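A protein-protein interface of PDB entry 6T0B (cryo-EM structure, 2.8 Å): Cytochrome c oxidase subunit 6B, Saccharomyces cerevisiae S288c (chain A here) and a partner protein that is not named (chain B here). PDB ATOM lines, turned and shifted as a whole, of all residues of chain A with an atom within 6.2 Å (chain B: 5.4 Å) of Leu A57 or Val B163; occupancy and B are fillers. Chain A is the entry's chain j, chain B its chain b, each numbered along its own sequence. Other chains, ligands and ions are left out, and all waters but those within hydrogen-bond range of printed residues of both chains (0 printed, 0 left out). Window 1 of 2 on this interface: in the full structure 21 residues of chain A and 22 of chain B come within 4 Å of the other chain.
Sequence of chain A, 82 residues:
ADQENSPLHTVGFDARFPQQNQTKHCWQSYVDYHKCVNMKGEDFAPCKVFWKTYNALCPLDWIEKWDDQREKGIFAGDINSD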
ATOM      1  N   VAL A  11     -21.180 -20.665 -28.397  1.00  0.00           N
ATOM      2  CA  VAL A  11     -19.920 -20.164 -28.924  1.00  0.00           C
ATOM      3  C   VAL A  11     -19.654 -20.723 -30.322  1.00  0.00           C
ATOM      4  O   VAL A  11     -19.758 -21.927 -30.575  1.00  0.00           O
ATOM      5  CB  VAL A  11     -18.792 -20.496 -27.928  1.00  0.00           C
ATOM      6  CG1 VAL A  11     -18.727 -21.987 -27.611  1.00  0.00           C
ATOM      7  CG2 VAL A  11     -17.465 -20.010 -28.429  1.00  0.00           C
ATOM      8  N   GLN A  22      -8.406 -25.859 -26.890  1.00  0.00           N
ATOM      9  CA  GLN A  22      -9.116 -24.610 -26.641  1.00  0.00           C
ATOM     10  C   GLN A  22      -8.928 -24.144 -25.205  1.00  0.00           C
ATOM     11  O   GLN A  22      -9.865 -23.655 -24.569  1.00  0.00           O
ATOM     12  CB  GLN A  22     -10.605 -24.756 -26.947  1.00  0.00           C
ATOM     13  CG  GLN A  22     -10.941 -25.042 -28.392  1.00  0.00           C
ATOM     14  CD  GLN A  22     -10.711 -23.853 -29.296  1.00  0.00           C
ATOM     15  OE1 GLN A  22     -10.995 -22.718 -28.928  1.00  0.00           O
ATOM     16  NE2 GLN A  22     -10.196 -24.109 -30.486  1.00  0.00           N
ATOM     17  N   THR A  23      -7.720 -24.303 -24.661  1.00  0.00           N
ATOM     18  CA  THR A  23      -7.460 -23.851 -23.296  1.00  0.00           C
ATOM     19  C   THR A  23      -7.377 -22.335 -23.237  1.00  0.00           C
ATOM     20  O   THR A  23      -7.994 -21.692 -22.373  1.00  0.00           O
ATOM     21  CB  THR A  23      -6.166 -24.466 -22.776  1.00  0.00           C
ATOM     22  OG1 THR A  23      -6.241 -25.884 -22.897  1.00  0.00           O
ATOM     23  CG2 THR A  23      -5.958 -24.110 -21.317  1.00  0.00           C
ATOM     24  N   HIS A  25      -8.837 -20.397 -25.137  1.00  0.00           N
ATOM     25  CA  HIS A  25     -10.113 -19.779 -25.451  1.00  0.00           C
ATOM     26  C   HIS A  25     -10.825 -19.380 -24.167  1.00  0.00           C
ATOM     27  O   HIS A  25     -11.202 -18.218 -23.986  1.00  0.00           O
ATOM     28  CB  HIS A  25     -10.974 -20.745 -26.269  1.00  0.00           C
ATOM     29  CG  HIS A  25     -11.952 -20.071 -27.179  1.00  0.00           C
ATOM     30  ND1 HIS A  25     -12.821 -20.775 -27.985  1.00  0.00           N
ATOM     31  CD2 HIS A  25     -12.203 -18.762 -27.409  1.00  0.00           C
ATOM     32  CE1 HIS A  25     -13.563 -19.928 -28.674  1.00  0.00           C
ATOM     33  NE2 HIS A  25     -13.208 -18.700 -28.344  1.00  0.00           N
ATOM     34  N   CYS A  26     -10.951 -20.326 -23.238  1.00  0.00           N
ATOM     35  CA  CYS A  26     -11.619 -20.028 -21.981  1.00  0.00           C
ATOM     36  C   CYS A  26     -10.748 -19.160 -21.089  1.00  0.00           C
ATOM     37  O   CYS A  26     -11.266 -18.257 -20.423  1.00  0.00           O
ATOM     38  CB  CYS A  26     -12.009 -21.316 -21.257  1.00  0.00           C
ATOM     39  SG  CYS A  26     -10.808 -21.960 -20.084  1.00  0.00           S
ATOM     40  N   LYS A  52     -20.147 -15.410 -21.816  1.00  0.00           N
ATOM     41  CA  LYS A  52     -20.698 -16.618 -22.422  1.00  0.00           C
ATOM     42  C   LYS A  52     -19.588 -17.500 -22.978  1.00  0.00           C
ATOM     43  O   LYS A  52     -19.657 -18.729 -22.860  1.00  0.00           O
ATOM     44  CB  LYS A  52     -21.748 -16.273 -23.496  1.00  0.00           C
ATOM     45  CG  LYS A  52     -21.298 -15.488 -24.735  1.00  0.00           C
ATOM     46  CD  LYS A  52     -20.896 -16.372 -25.930  1.00  0.00           C
ATOM     47  CE  LYS A  52     -20.442 -15.540 -27.124  1.00  0.00           C
ATOM     48  NZ  LYS A  52     -19.967 -16.375 -28.266  1.00  0.00           N
ATOM     49  N   THR A  53     -18.516 -16.889 -23.500  1.00  0.00           N
ATOM     50  CA  THR A  53     -17.441 -17.676 -24.088  1.00  0.00           C
ATOM     51  C   THR A  53     -16.665 -18.453 -23.031  1.00  0.00           C
ATOM     52  O   THR A  53     -16.362 -19.635 -23.230  1.00  0.00           O
ATOM     53  CB  THR A  53     -16.503 -16.775 -24.885  1.00  0.00           C
ATOM     54  OG1 THR A  53     -17.265 -16.024 -25.833  1.00  0.00           O
ATOM     55  CG2 THR A  53     -15.516 -17.619 -25.664  1.00  0.00           C
ATOM     56  N   TYR A  54     -16.349 -17.830 -21.892  1.00  0.00           N
ATOM     57  CA  TYR A  54     -15.606 -18.594 -20.895  1.00  0.00           C
ATOM     58  C   TYR A  54     -16.489 -19.534 -20.093  1.00  0.00           C
ATOM     59  O   TYR A  54     -16.044 -20.640 -19.774  1.00  0.00           O
ATOM     60  CB  TYR A  54     -14.765 -17.691 -19.963  1.00  0.00           C
ATOM     61  CG  TYR A  54     -15.401 -16.907 -18.808  1.00  0.00           C
ATOM     62  CD1 TYR A  54     -15.736 -17.512 -17.598  1.00  0.00           C
ATOM     63  CD2 TYR A  54     -15.534 -15.535 -18.889  1.00  0.00           C
ATOM     64  CE1 TYR A  54     -16.269 -16.781 -16.558  1.00  0.00           C
ATOM     65  CE2 TYR A  54     -16.065 -14.805 -17.856  1.00  0.00           C
ATOM     66  CZ  TYR A  54     -16.426 -15.428 -16.697  1.00  0.00           C
ATOM     67  OH  TYR A  54     -16.949 -14.676 -15.677  1.00  0.00           O
ATOM     68  N   ASN A  55     -17.728 -19.163 -19.780  1.00  0.00           N
ATOM     69  CA  ASN A  55     -18.542 -20.092 -19.017  1.00  0.00           C
ATOM     70  C   ASN A  55     -19.186 -21.177 -19.874  1.00  0.00           C
ATOM     71  O   ASN A  55     -19.738 -22.128 -19.313  1.00  0.00           O
ATOM     72  CB  ASN A  55     -19.610 -19.339 -18.222  1.00  0.00           C
ATOM     73  CG  ASN A  55     -19.727 -19.847 -16.806  1.00  0.00           C
ATOM     74  OD1 ASN A  55     -18.788 -20.429 -16.270  1.00  0.00           O
ATOM     75  ND2 ASN A  55     -20.873 -19.623 -16.186  1.00  0.00           N
ATOM     76  N   ALA A  56     -19.106 -21.092 -21.204  1.00  0.00           N
ATOM     77  CA  ALA A  56     -19.658 -22.166 -22.016  1.00  0.00           C
ATOM     78  C   ALA A  56     -18.668 -23.306 -22.203  1.00  0.00           C
ATOM     79  O   ALA A  56     -19.077 -24.466 -22.315  1.00  0.00           O
ATOM     80  CB  ALA A  56     -20.100 -21.619 -23.373  1.00  0.00           C
ATOM     81  N   LEU A  57     -17.369 -23.013 -22.226  1.00  0.00           N
ATOM     82  CA  LEU A  57     -16.390 -24.060 -22.475  1.00  0.00           C
ATOM     83  C   LEU A  57     -15.272 -24.113 -21.441  1.00  0.00           C
ATOM     84  O   LEU A  57     -14.281 -24.822 -21.664  1.00  0.00           O
ATOM     85  CB  LEU A  57     -15.799 -23.924 -23.883  1.00  0.00           C
ATOM     86  CG  LEU A  57     -15.042 -22.697 -24.378  1.00  0.00           C
ATOM     87  CD1 LEU A  57     -13.546 -22.867 -24.245  1.00  0.00           C
ATOM     88  CD2 LEU A  57     -15.400 -22.461 -25.823  1.00  0.00           C
ATOM     89  N   CYS A  58     -15.404 -23.424 -20.304  1.00  0.00           N
ATOM     90  CA  CYS A  58     -14.320 -23.655 -19.369  1.00  0.00           C
ATOM     91  C   CYS A  58     -14.873 -24.254 -18.080  1.00  0.00           C
ATOM     92  O   CYS A  58     -15.922 -23.812 -17.602  1.00  0.00           O
ATOM     93  CB  CYS A  58     -13.580 -22.349 -19.063  1.00  0.00           C
ATOM     94  SG  CYS A  58     -11.874 -22.502 -18.468  1.00  0.00           S
ATOM     95  N   PRO A  59     -14.217 -25.262 -17.513  1.00  0.00           N
ATOM     96  CA  PRO A  59     -14.845 -26.038 -16.442  1.00  0.00           C
ATOM     97  C   PRO A  59     -14.867 -25.321 -15.099  1.00  0.00           C
ATOM     98  O   PRO A  59     -14.110 -24.381 -14.828  1.00  0.00           O
ATOM     99  CB  PRO A  59     -14.012 -27.321 -16.401  1.00  0.00           C
ATOM    100  CG  PRO A  59     -12.760 -26.994 -17.074  1.00  0.00           C
ATOM    101  CD  PRO A  59     -13.061 -25.963 -18.086  1.00  0.00           C
ATOM    102  N   THR B 101     -22.791 -26.832 -26.728  1.00  0.00           N
ATOM    103  CA  THR B 101     -21.550 -27.294 -26.136  1.00  0.00           C
ATOM    104  C   THR B 101     -21.848 -28.136 -24.904  1.00  0.00           C
ATOM    105  O   THR B 101     -22.840 -27.919 -24.204  1.00  0.00           O
ATOM    106  CB  THR B 101     -20.614 -26.134 -25.794  1.00  0.00           C
ATOM    107  OG1 THR B 101     -19.346 -26.656 -25.389  1.00  0.00           O
ATOM    108  CG2 THR B 101     -21.181 -25.239 -24.707  1.00  0.00           C
ATOM    109  N   ILE B 102     -21.027 -29.159 -24.692  1.00  0.00           N
ATOM    110  CA  ILE B 102     -21.112 -30.019 -23.519  1.00  0.00           C
ATOM    111  C   ILE B 102     -19.701 -30.278 -23.041  1.00  0.00           C
ATOM    112  O   ILE B 102     -18.866 -30.751 -23.813  1.00  0.00           O
ATOM    113  CB  ILE B 102     -21.797 -31.370 -23.793  1.00  0.00           C
ATOM    114  CG1 ILE B 102     -23.229 -31.208 -24.277  1.00  0.00           C
ATOM    115  CG2 ILE B 102     -21.815 -32.208 -22.544  1.00  0.00           C
ATOM    116  CD1 ILE B 102     -23.381 -31.486 -25.723  1.00  0.00           C
ATOM    117  N   LYS B 103     -19.426 -29.983 -21.778  1.00  0.00           N
ATOM    118  CA  LYS B 103     -18.143 -30.325 -21.207  1.00  0.00           C
ATOM    119  C   LYS B 103     -18.210 -31.661 -20.501  1.00  0.00           C
ATOM    120  O   LYS B 103     -19.191 -31.970 -19.824  1.00  0.00           O
ATOM    121  CB  LYS B 103     -17.680 -29.252 -20.245  1.00  0.00           C
ATOM    122  CG  LYS B 103     -17.294 -28.004 -20.952  1.00  0.00           C
ATOM    123  CD  LYS B 103     -16.536 -27.112 -20.039  1.00  0.00           C
ATOM    124  CE  LYS B 103     -17.403 -26.715 -18.883  1.00  0.00           C
ATOM    125  NZ  LYS B 103     -18.386 -25.654 -19.176  1.00  0.00           N
ATOM    126  N   ALA B 104     -17.161 -32.450 -20.662  1.00  0.00           N
ATOM    127  CA  ALA B 104     -17.067 -33.759 -20.035  1.00  0.00           C
ATOM    128  C   ALA B 104     -15.740 -33.818 -19.306  1.00  0.00           C
ATOM    129  O   ALA B 104     -14.686 -33.751 -19.939  1.00  0.00           O
ATOM    130  CB  ALA B 104     -17.177 -34.873 -21.066  1.00  0.00           C
ATOM    131  N   SER B 116     -23.525 -26.062 -20.599  1.00  0.00           N
ATOM    132  CA  SER B 116     -23.062 -24.770 -20.118  1.00  0.00           C
ATOM    133  C   SER B 116     -23.549 -23.618 -20.982  1.00  0.00           C
ATOM    134  O   SER B 116     -22.872 -22.599 -21.096  1.00  0.00           O
ATOM    135  CB  SER B 116     -21.541 -24.762 -20.043  1.00  0.00           C
ATOM    136  OG  SER B 116     -20.979 -25.212 -21.259  1.00  0.00           O
ATOM    137  N   ARG B 161     -20.663 -29.821 -29.738  1.00  0.00           N
ATOM    138  CA  ARG B 161     -19.230 -29.694 -29.535  1.00  0.00           C
ATOM    139  C   ARG B 161     -18.909 -30.188 -28.136  1.00  0.00           C
ATOM    140  O   ARG B 161     -19.364 -29.611 -27.146  1.00  0.00           O
ATOM    141  CB  ARG B 161     -18.764 -28.260 -29.727  1.00  0.00           C
ATOM    142  CG  ARG B 161     -17.388 -28.000 -29.171  1.00  0.00           C
ATOM    143  CD  ARG B 161     -17.062 -26.521 -29.183  1.00  0.00           C
ATOM    144  NE  ARG B 161     -16.844 -26.041 -30.543  1.00  0.00           N
ATOM    145  CZ  ARG B 161     -17.110 -24.814 -30.963  1.00  0.00           C
ATOM    146  NH1 ARG B 161     -17.616 -23.939 -30.123  1.00  0.00           N
ATOM    147  NH2 ARG B 161     -16.875 -24.481 -32.222  1.00  0.00           N
ATOM    148  N   PHE B 162     -18.154 -31.271 -28.060  1.00  0.00           N
ATOM    149  CA  PHE B 162     -17.720 -31.832 -26.793  1.00  0.00           C
ATOM    150  C   PHE B 162     -16.371 -31.237 -26.440  1.00  0.00           C
ATOM    151  O   PHE B 162     -15.404 -31.408 -27.186  1.00  0.00           O
ATOM    152  CB  PHE B 162     -17.612 -33.349 -26.881  1.00  0.00           C
ATOM    153  CG  PHE B 162     -18.926 -34.041 -26.987  1.00  0.00           C
ATOM    154  CD1 PHE B 162     -19.852 -33.935 -25.979  1.00  0.00           C
ATOM    155  CD2 PHE B 162     -19.231 -34.804 -28.087  1.00  0.00           C
ATOM    156  CE1 PHE B 162     -21.057 -34.572 -26.070  1.00  0.00           C
ATOM    157  CE2 PHE B 162     -20.435 -35.443 -28.177  1.00  0.00           C
ATOM    158  CZ  PHE B 162     -21.342 -35.328 -27.168  1.00  0.00           C
ATOM    159  N   VAL B 163     -16.312 -30.532 -25.320  1.00  0.00           N
ATOM    160  CA  VAL B 163     -15.072 -30.000 -24.783  1.00  0.00           C
ATOM    161  C   VAL B 163     -14.650 -30.901 -23.639  1.00  0.00           C
ATOM    162  O   VAL B 163     -15.374 -31.046 -22.654  1.00  0.00           O
ATOM    163  CB  VAL B 163     -15.237 -28.554 -24.313  1.00  0.00           C
ATOM    164  CG1 VAL B 163     -13.894 -27.965 -24.015  1.00  0.00           C
ATOM    165  CG2 VAL B 163     -15.955 -27.746 -25.358  1.00  0.00           C
ATOM    166  N   VAL B 164     -13.485 -31.508 -23.755  1.00  0.00           N
ATOM    167  CA  VAL B 164     -13.112 -32.630 -22.916  1.00  0.00           C
ATOM    168  C   VAL B 164     -11.848 -32.275 -22.153  1.00  0.00           C
ATOM    169  O   VAL B 164     -10.873 -31.796 -22.743  1.00  0.00           O
ATOM    170  CB  VAL B 164     -12.934 -33.898 -23.766  1.00  0.00           C
ATOM    171  CG1 VAL B 164     -12.298 -34.975 -22.986  1.00  0.00           C
ATOM    172  CG2 VAL B 164     -14.277 -34.367 -24.244  1.00  0.00           C
ATOM    173  N   THR B 165     -11.888 -32.473 -20.834  1.00  0.00           N
ATOM    174  CA  THR B 165     -10.730 -32.311 -19.973  1.00  0.00           C
ATOM    175  C   THR B 165     -10.846 -33.292 -18.824  1.00  0.00           C
ATOM    176  O   THR B 165     -11.770 -34.099 -18.766  1.00  0.00           O
ATOM    177  CB  THR B 165     -10.624 -30.896 -19.447  1.00  0.00           C
ATOM    178  OG1 THR B 165      -9.453 -30.783 -18.641  1.00  0.00           O
ATOM    179  CG2 THR B 165     -11.821 -30.568 -18.620  1.00  0.00           C
ATOM    180  N   LEU B 189      -7.989 -28.476 -22.707  1.00  0.00           N
ATOM    181  CA  LEU B 189      -9.349 -28.682 -23.178  1.00  0.00           C
ATOM    182  C   LEU B 189      -9.300 -29.047 -24.646  1.00  0.00           C
ATOM    183  O   LEU B 189      -8.936 -28.211 -25.474  1.00  0.00           O
ATOM    184  CB  LEU B 189     -10.184 -27.422 -23.017  1.00  0.00           C
ATOM    185  CG  LEU B 189     -10.457 -26.859 -21.642  1.00  0.00           C
ATOM    186  CD1 LEU B 189     -10.890 -25.430 -21.794  1.00  0.00           C
ATOM    187  CD2 LEU B 189     -11.546 -27.656 -21.009  1.00  0.00           C
ATOM    188  N   ASN B 190      -9.699 -30.262 -24.978  1.00  0.00           N
ATOM    189  CA  ASN B 190      -9.853 -30.614 -26.377  1.00  0.00           C
ATOM    190  C   ASN B 190     -11.308 -30.461 -26.790  1.00  0.00           C
ATOM    191  O   ASN B 190     -12.202 -30.336 -25.960  1.00  0.00           O
ATOM    192  CB  ASN B 190      -9.378 -32.032 -26.638  1.00  0.00           C
ATOM    193  CG  ASN B 190      -7.999 -32.270 -26.146  1.00  0.00           C
ATOM    194  OD1 ASN B 190      -7.209 -31.345 -26.026  1.00  0.00           O
ATOM    195  ND2 ASN B 190      -7.687 -33.517 -25.856  1.00  0.00           N
ATOM    196  N   GLN B 191     -11.546 -30.476 -28.091  1.00  0.00           N
ATOM    197  CA  GLN B 191     -12.910 -30.444 -28.580  1.00  0.00           C
ATOM    198  C   GLN B 191     -13.052 -31.427 -29.721  1.00  0.00           C
ATOM    199  O   GLN B 191     -12.106 -31.664 -30.475  1.00  0.00           O
ATOM    200  CB  GLN B 191     -13.315 -29.052 -29.040  1.00  0.00           C
ATOM    201  CG  GLN B 191     -12.434 -28.473 -30.091  1.00  0.00           C
ATOM    202  CD  GLN B 191     -12.872 -27.108 -30.510  1.00  0.00           C
ATOM    203  OE1 GLN B 191     -13.906 -26.623 -30.077  1.00  0.00           O
ATOM    204  NE2 GLN B 191     -12.077 -26.465 -31.356  1.00  0.00           N
ATOM    205  N   VAL B 192     -14.224 -32.045 -29.802  1.00  0.00           N
ATOM    206  CA  VAL B 192     -14.652 -32.796 -30.973  1.00  0.00           C
ATOM    207  C   VAL B 192     -16.057 -32.328 -31.313  1.00  0.00           C
ATOM    208  O   VAL B 192     -16.722 -31.674 -30.511  1.00  0.00           O
ATOM    209  CB  VAL B 192     -14.632 -34.320 -30.759  1.00  0.00           C
ATOM    210  CG1 VAL B 192     -13.253 -34.810 -30.372  1.00  0.00           C
ATOM    211  CG2 VAL B 192     -15.625 -34.702 -29.708  1.00  0.00           C
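The side-chain amino group (NZ) of Lys B103 lies within hydrogen-bond range of the backbone carbonyl oxygen (O) of Cys A58. The backbone carbonyl oxygen (O) of Val A11 sits at hydrogen-bond distance from the guanidinium group (NH1) of Arg B161 (3.0 Å). The side-chain hydroxyl (OG) of Ser B116 sits close to the backbone carbonyl oxygen (O) of Ala A56 (2.3 Å). The backbone NH (N) of Leu B189 lies within hydrogen-bond range of the side-chain hydroxyl (OG1) of Thr A23 (3.1 Å). The side-chain amide nitrogen (NE2) of Gln A22 sits close to the side-chain amide nitrogen (NE2) of Gln B191 (3.1 Å). N of Gln A22 is in hydrogen-bond range of O of Leu B189 (2.8 Å). O of Ala A56 lies within hydrogen-bond range of NZ of Lys B103.
Printed residues of chain B within 4 Å of Gln A22: Leu B189 and Gln B191. Printed residues of chain B within 4 Å of Thr A23: Leu B189. Leu A57 touches just these residues of chain B: Lys B103 (3.5 Å), Val B163 (3.9 Å) and Leu B189 (3.4 Å). Of chain A, only Leu A57 comes within 4 Å of Val B163. The nearest residue of chain B that does not touch Leu A57 is Ser B116 (4.3 Å). The nearest printed residue of chain A that does not touch Val B163 is Gln A22 (5.5 Å). The nearest printed residue of chain A that does not touch Lys B103 is Tyr A54 (5.6 Å).
Printed residues of chain A that touch a printed residue of chain B: Val A11, Gln A22, Thr A23, Cys A26, Asn A55, Ala A56, Leu A57, Cys A58 and Pro A59. Hydrophobic or aromatic side chains of chain A that line the printed part of chain B: Val A11, Ala A56 and Pro A59. Among the printed residues, 16 pairs touch across the chains. Among the printed residues, no Asp or Glu carboxylate lies within 4 Å of a Lys or Arg side-chain nitrogen of the other chain.
The side-chain amide oxygen (OE1) of Gln A22 is in hydrogen-bond range of a ring nitrogen (ND1) of His A25 (2.8 Å). The backbone NH of Val B163 lies within hydrogen-bond range of the backbone carbonyl oxygen of Ile B102 (3.0 Å). The side-chain sulfur of Cys A26 forms a disulfide with the side-chain sulfur of Cys A58, at 2.0 Å. The side-chain amino group of Lys B103 is in hydrogen-bond range of the side-chain hydroxyl of Ser B116 (3.4 Å). OE1 of Gln B191 is in hydrogen-bond range of NE of Arg B161. The side-chain hydroxyl (OG1) of Thr B101 sits close to the backbone carbonyl oxygen (O) of Arg B161, at 3.4 Å.
Among the printed residues, merely in contact across the chains: Asn A55 with Ser B116 (3.3 Å), Ala A56 with Thr B101 (3.3 Å), Leu A57 with Leu B189 (3.4 Å), Leu A57 with Lys B103 (3.5 Å), Pro A59 with Lys B103 (3.6 Å), Pro A59 with Leu B189 (3.7 Å), Asn A55 with Lys B103 (3.8 Å), Cys A26 with Leu B189 (3.9 Å) and Leu A57 with Val B163 (3.9 Å).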
